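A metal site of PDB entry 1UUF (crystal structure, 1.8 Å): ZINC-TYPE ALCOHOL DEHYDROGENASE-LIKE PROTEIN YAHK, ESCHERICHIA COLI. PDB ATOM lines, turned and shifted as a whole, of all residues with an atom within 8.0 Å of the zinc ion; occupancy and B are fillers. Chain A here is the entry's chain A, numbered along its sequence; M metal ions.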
ATOM      1  N   ASP A 111      11.197   1.017 -20.540  1.00  0.00           N
ATOM      2  CA  ASP A 111      11.466   1.358 -19.140  1.00  0.00           C
ATOM      3  C   ASP A 111      12.774   2.143 -19.003  1.00  0.00           C
ATOM      4  O   ASP A 111      13.586   2.188 -19.925  1.00  0.00           O
ATOM      5  CB  ASP A 111      11.540   0.083 -18.287  1.00  0.00           C
ATOM      6  CG  ASP A 111      11.047   0.306 -16.850  1.00  0.00           C
ATOM      7  OD1 ASP A 111      10.791   1.475 -16.481  1.00  0.00           O
ATOM      8  OD2 ASP A 111      10.914  -0.681 -16.098  1.00  0.00           O
ATOM      9  N   SER A 112      12.937   2.799 -17.861  1.00  0.00           N
ATOM     10  CA  SER A 112      14.154   3.559 -17.577  1.00  0.00           C
ATOM     11  C   SER A 112      14.264   3.669 -16.057  1.00  0.00           C
ATOM     12  O   SER A 112      13.342   3.289 -15.336  1.00  0.00           O
ATOM     13  CB  SER A 112      14.124   4.937 -18.239  1.00  0.00           C
ATOM     14  OG  SER A 112      13.115   5.778 -17.709  1.00  0.00           O
ATOM     15  N   CYS A 113      15.380   4.196 -15.554  1.00  0.00           N
ATOM     16  CA  CYS A 113      15.558   4.287 -14.109  1.00  0.00           C
ATOM     17  C   CYS A 113      14.577   5.236 -13.415  1.00  0.00           C
ATOM     18  O   CYS A 113      14.240   5.041 -12.252  1.00  0.00           O
ATOM     19  CB  CYS A 113      17.000   4.647 -13.763  1.00  0.00           C
ATOM     20  SG  CYS A 113      17.412   6.401 -13.686  1.00  0.00           S
ATOM     21  N   LYS A 114      14.117   6.253 -14.149  1.00  0.00           N
ATOM     22  CA  LYS A 114      13.160   7.230 -13.650  1.00  0.00           C
ATOM     23  C   LYS A 114      13.648   8.220 -12.596  1.00  0.00           C
ATOM     24  O   LYS A 114      12.865   9.038 -12.124  1.00  0.00           O
ATOM     25  CB  LYS A 114      11.919   6.532 -13.086  1.00  0.00           C
ATOM     26  CG  LYS A 114      11.281   5.528 -14.021  1.00  0.00           C
ATOM     27  CD  LYS A 114      10.078   4.881 -13.349  1.00  0.00           C
ATOM     28  CE  LYS A 114       9.665   3.622 -14.081  1.00  0.00           C
ATOM     29  NZ  LYS A 114      10.769   2.628 -14.035  1.00  0.00           N
ATOM     30  N   HIS A 115      14.921   8.161 -12.228  1.00  0.00           N
ATOM     31  CA  HIS A 115      15.394   9.098 -11.206  1.00  0.00           C
ATOM     32  C   HIS A 115      16.691   9.838 -11.524  1.00  0.00           C
ATOM     33  O   HIS A 115      17.186  10.589 -10.689  1.00  0.00           O
ATOM     34  CB  HIS A 115      15.528   8.365  -9.861  1.00  0.00           C
ATOM     35  CG  HIS A 115      16.474   7.209  -9.888  1.00  0.00           C
ATOM     36  ND1 HIS A 115      17.839   7.352  -9.753  1.00  0.00           N
ATOM     37  CD2 HIS A 115      16.251   5.883 -10.038  1.00  0.00           C
ATOM     38  CE1 HIS A 115      18.415   6.173  -9.827  1.00  0.00           C
ATOM     39  NE2 HIS A 115      17.480   5.258 -10.006  1.00  0.00           N
ATOM     40  N   CYS A 116      17.244   9.629 -12.715  1.00  0.00           N
ATOM     41  CA  CYS A 116      18.463  10.312 -13.101  1.00  0.00           C
ATOM     42  C   CYS A 116      18.096  11.638 -13.768  1.00  0.00           C
ATOM     43  O   CYS A 116      16.921  11.886 -14.051  1.00  0.00           O
ATOM     44  CB  CYS A 116      19.296   9.471 -14.063  1.00  0.00           C
ATOM     45  SG  CYS A 116      18.592   9.352 -15.725  1.00  0.00           S
ATOM     46  N   GLU A 117      19.085  12.481 -14.031  1.00  0.00           N
ATOM     47  CA  GLU A 117      18.833  13.768 -14.647  1.00  0.00           C
ATOM     48  C   GLU A 117      18.094  13.635 -15.980  1.00  0.00           C
ATOM     49  O   GLU A 117      17.176  14.403 -16.263  1.00  0.00           O
ATOM     50  CB  GLU A 117      20.152  14.513 -14.861  1.00  0.00           C
ATOM     51  CG  GLU A 117      19.965  15.957 -15.328  1.00  0.00           C
ATOM     52  CD  GLU A 117      21.280  16.696 -15.455  1.00  0.00           C
ATOM     53  OE1 GLU A 117      22.051  16.727 -14.469  1.00  0.00           O
ATOM     54  OE2 GLU A 117      21.549  17.260 -16.544  1.00  0.00           O
ATOM     55  N   GLU A 118      18.487  12.664 -16.792  1.00  0.00           N
ATOM     56  CA  GLU A 118      17.853  12.462 -18.088  1.00  0.00           C
ATOM     57  C   GLU A 118      16.374  12.092 -17.965  1.00  0.00           C
ATOM     58  O   GLU A 118      15.523  12.706 -18.607  1.00  0.00           O
ATOM     59  CB  GLU A 118      18.600  11.368 -18.869  1.00  0.00           C
ATOM     60  CG  GLU A 118      19.896  11.851 -19.519  1.00  0.00           C
ATOM     61  CD  GLU A 118      20.880  12.431 -18.523  1.00  0.00           C
ATOM     62  OE1 GLU A 118      21.376  11.665 -17.656  1.00  0.00           O
ATOM     63  OE2 GLU A 118      21.169  13.641 -18.597  1.00  0.00           O
ATOM     64  N   CYS A 119      16.070  11.094 -17.146  1.00  0.00           N
ATOM     65  CA  CYS A 119      14.685  10.674 -16.964  1.00  0.00           C
ATOM     66  C   CYS A 119      13.822  11.804 -16.399  1.00  0.00           C
ATOM     67  O   CYS A 119      12.683  11.998 -16.834  1.00  0.00           O
ATOM     68  CB  CYS A 119      14.614   9.457 -16.038  1.00  0.00           C
ATOM     69  SG  CYS A 119      15.191   7.929 -16.820  1.00  0.00           S
ATOM     70  N   GLU A 120      14.371  12.551 -15.447  1.00  0.00           N
ATOM     71  CA  GLU A 120      13.619  13.648 -14.843  1.00  0.00           C
ATOM     72  C   GLU A 120      13.389  14.796 -15.833  1.00  0.00           C
ATOM     73  O   GLU A 120      12.475  15.595 -15.650  1.00  0.00           O
ATOM     74  CB  GLU A 120      14.349  14.151 -13.590  1.00  0.00           C
ATOM     75  CG  GLU A 120      14.538  13.062 -12.544  1.00  0.00           C
ATOM     76  CD  GLU A 120      15.099  13.589 -11.246  1.00  0.00           C
ATOM     77  OE1 GLU A 120      16.128  14.293 -11.274  1.00  0.00           O
ATOM     78  OE2 GLU A 120      14.508  13.289 -10.185  1.00  0.00           O
ATOM     79  N   LEU A 123      13.920  12.772 -20.847  1.00  0.00           N
ATOM     80  CA  LEU A 123      14.846  12.231 -21.836  1.00  0.00           C
ATOM     81  C   LEU A 123      15.223  10.794 -21.468  1.00  0.00           C
ATOM     82  O   LEU A 123      16.403  10.457 -21.355  1.00  0.00           O
ATOM     83  CB  LEU A 123      16.099  13.104 -21.926  1.00  0.00           C
ATOM     84  CG  LEU A 123      15.870  14.534 -22.407  1.00  0.00           C
ATOM     85  CD1 LEU A 123      17.166  15.324 -22.313  1.00  0.00           C
ATOM     86  CD2 LEU A 123      15.361  14.520 -23.854  1.00  0.00           C
ATOM     87  N   GLU A 124      14.211   9.953 -21.279  1.00  0.00           N
ATOM     88  CA  GLU A 124      14.444   8.557 -20.921  1.00  0.00           C
ATOM     89  C   GLU A 124      15.309   7.856 -21.963  1.00  0.00           C
ATOM     90  O   GLU A 124      15.959   6.846 -21.663  1.00  0.00           O
ATOM     91  CB  GLU A 124      13.113   7.831 -20.767  1.00  0.00           C
ATOM     92  CG  GLU A 124      12.219   8.414 -19.690  1.00  0.00           C
ATOM     93  CD  GLU A 124      11.224   9.445 -20.208  1.00  0.00           C
ATOM     94  OE1 GLU A 124      11.454  10.032 -21.293  1.00  0.00           O
ATOM     95  OE2 GLU A 124      10.215   9.673 -19.520  1.00  0.00           O
ATOM     96  N   ASN A 125      15.337   8.395 -23.181  1.00  0.00           N
ATOM     97  CA  ASN A 125      16.131   7.811 -24.259  1.00  0.00           C
ATOM     98  C   ASN A 125      17.641   7.922 -24.020  1.00  0.00           C
ATOM     99  O   ASN A 125      18.424   7.145 -24.568  1.00  0.00           O
ATOM    100  CB  ASN A 125      15.760   8.472 -25.603  1.00  0.00           C
ATOM    101  CG  ASN A 125      15.865   9.992 -25.568  1.00  0.00           C
ATOM    102  OD1 ASN A 125      15.449  10.640 -24.611  1.00  0.00           O
ATOM    103  ND2 ASN A 125      16.405  10.571 -26.641  1.00  0.00           N
ATOM    104  N   TYR A 126      18.038   8.886 -23.196  1.00  0.00           N
ATOM    105  CA  TYR A 126      19.445   9.082 -22.887  1.00  0.00           C
ATOM    106  C   TYR A 126      19.827   8.546 -21.505  1.00  0.00           C
ATOM    107  O   TYR A 126      20.921   8.775 -21.014  1.00  0.00           O
ATOM    108  CB  TYR A 126      19.810  10.569 -22.997  1.00  0.00           C
ATOM    109  CG  TYR A 126      19.733  11.081 -24.417  1.00  0.00           C
ATOM    110  CD1 TYR A 126      18.907  12.155 -24.755  1.00  0.00           C
ATOM    111  CD2 TYR A 126      20.448  10.456 -25.440  1.00  0.00           C
ATOM    112  CE1 TYR A 126      18.799  12.593 -26.076  1.00  0.00           C
ATOM    113  CE2 TYR A 126      20.341  10.880 -26.760  1.00  0.00           C
ATOM    114  CZ  TYR A 126      19.521  11.942 -27.074  1.00  0.00           C
ATOM    115  OH  TYR A 126      19.387  12.318 -28.388  1.00  0.00           O
ATOM    116  N   CYS A 127      18.906   7.827 -20.881  1.00  0.00           N
ATOM    117  CA  CYS A 127      19.149   7.239 -19.566  1.00  0.00           C
ATOM    118  C   CYS A 127      20.213   6.142 -19.729  1.00  0.00           C
ATOM    119  O   CYS A 127      20.156   5.370 -20.688  1.00  0.00           O
ATOM    120  CB  CYS A 127      17.863   6.642 -19.003  1.00  0.00           C
ATOM    121  SG  CYS A 127      18.044   5.683 -17.469  1.00  0.00           S
ATOM    122  N   ASP A 128      21.166   6.078 -18.804  1.00  0.00           N
ATOM    123  CA  ASP A 128      22.203   5.050 -18.884  1.00  0.00           C
ATOM    124  C   ASP A 128      21.650   3.659 -18.638  1.00  0.00           C
ATOM    125  O   ASP A 128      22.292   2.664 -18.973  1.00  0.00           O
ATOM    126  CB  ASP A 128      23.313   5.299 -17.855  1.00  0.00           C
ATOM    127  CG  ASP A 128      24.301   6.346 -18.305  1.00  0.00           C
ATOM    128  OD1 ASP A 128      24.581   6.431 -19.520  1.00  0.00           O
ATOM    129  OD2 ASP A 128      24.812   7.079 -17.426  1.00  0.00           O
ATOM    130  N   HIS A 129      20.475   3.595 -18.049  1.00  0.00           N
ATOM    131  CA  HIS A 129      19.871   2.305 -17.729  1.00  0.00           C
ATOM    132  C   HIS A 129      18.510   2.138 -18.393  1.00  0.00           C
ATOM    133  O   HIS A 129      17.610   1.522 -17.834  1.00  0.00           O
ATOM    134  CB  HIS A 129      19.751   2.179 -16.214  1.00  0.00           C
ATOM    135  CG  HIS A 129      21.021   2.490 -15.501  1.00  0.00           C
ATOM    136  ND1 HIS A 129      22.148   1.705 -15.597  1.00  0.00           N
ATOM    137  CD2 HIS A 129      21.385   3.556 -14.746  1.00  0.00           C
ATOM    138  CE1 HIS A 129      23.137   2.257 -14.935  1.00  0.00           C
ATOM    139  NE2 HIS A 129      22.705   3.389 -14.405  1.00  0.00           N
ATOM    140  N   MET A 130      18.385   2.689 -19.592  1.00  0.00           N
ATOM    141  CA  MET A 130      17.138   2.582 -20.333  1.00  0.00           C
ATOM    142  C   MET A 130      16.946   1.147 -20.801  1.00  0.00           C
ATOM    143  O   MET A 130      17.897   0.492 -21.251  1.00  0.00           O
ATOM    144  CB  MET A 130      17.181   3.539 -21.537  1.00  0.00           C
ATOM    145  CG  MET A 130      15.919   3.541 -22.380  1.00  0.00           C
ATOM    146  SD  MET A 130      16.027   2.429 -23.787  1.00  0.00           S
ATOM    147  CE  MET A 130      16.915   3.482 -24.937  1.00  0.00           C
ATOM    148  N   ARG A 158       4.073   4.697 -18.337  1.00  0.00           N
ATOM    149  CA  ARG A 158       4.897   5.880 -18.569  1.00  0.00           C
ATOM    150  C   ARG A 158       5.521   5.858 -19.956  1.00  0.00           C
ATOM    151  O   ARG A 158       5.832   6.911 -20.527  1.00  0.00           O
ATOM    152  CB  ARG A 158       6.016   5.988 -17.511  1.00  0.00           C
ATOM    153  CG  ARG A 158       7.058   7.074 -17.838  1.00  0.00           C
ATOM    154  CD  ARG A 158       8.003   7.322 -16.665  1.00  0.00           C
ATOM    155  NE  ARG A 158       9.021   8.326 -16.998  1.00  0.00           N
ATOM    156  CZ  ARG A 158       9.788   8.921 -16.089  1.00  0.00           C
ATOM    157  NH1 ARG A 158       9.662   8.632 -14.806  1.00  0.00           N
ATOM    158  NH2 ARG A 158      10.697   9.821 -16.467  1.00  0.00           N
ATOM    159  N   TYR A 159       5.674   4.668 -20.515  1.00  0.00           N
ATOM    160  CA  TYR A 159       6.293   4.532 -21.822  1.00  0.00           C
ATOM    161  C   TYR A 159       5.338   4.197 -22.957  1.00  0.00           C
ATOM    162  O   TYR A 159       5.765   3.863 -24.061  1.00  0.00           O
ATOM    163  CB  TYR A 159       7.424   3.493 -21.725  1.00  0.00           C
ATOM    164  CG  TYR A 159       8.342   3.787 -20.562  1.00  0.00           C
ATOM    165  CD1 TYR A 159       8.037   3.320 -19.273  1.00  0.00           C
ATOM    166  CD2 TYR A 159       9.450   4.607 -20.727  1.00  0.00           C
ATOM    167  CE1 TYR A 159       8.820   3.684 -18.187  1.00  0.00           C
ATOM    168  CE2 TYR A 159      10.246   4.966 -19.639  1.00  0.00           C
ATOM    169  CZ  TYR A 159       9.924   4.504 -18.376  1.00  0.00           C
ATOM    170  OH  TYR A 159      10.698   4.881 -17.298  1.00  0.00           O
HETATM  171 ZN    ZN M   1      17.362   7.311 -15.865  1.00  0.00          ZN
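The side-chain sulfur (SG) of Cys 113 sits close to the backbone NH (N) of His 115 (3.4 Å).
The side-chain sulfur (SG) of Cys 127 sits close to the backbone NH (N) of Met 130 (3.7 Å).
N of Glu 118 sits close to SG of Cys 116, at 3.5 Å.
The side-chain sulfur (SG) of Cys 119 sits close to the backbone NH (N) of Lys 114, 3.3 Å away.
SG of Cys 119 sits close to OG of Ser 112 (3.1 Å).
O of Cys 119 lies within hydrogen-bond range of NH2 of Arg 158 (3.0 Å).
The side-chain amino group (NZ) of Lys 114 lies within hydrogen-bond range of the backbone carbonyl oxygen (O) of Ser 112 (3.0 Å).
OD1 of Asp 111 is in salt-bridge range of NZ of Lys 114 (2.7 Å).
Merely in contact with the zinc ion: Lys 114.
Of the 20 residues printed, 5 come within 4 Å of the zinc ion.
Along chain A the residues within 4 Å of the zinc ion span positions 113 to 127.
The zinc ion is bound by the side-chain sulfur of Cys 113, the side-chain sulfur of Cys 127, the side-chain sulfur of Cys 116 and the side-chain sulfur of Cys 119.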
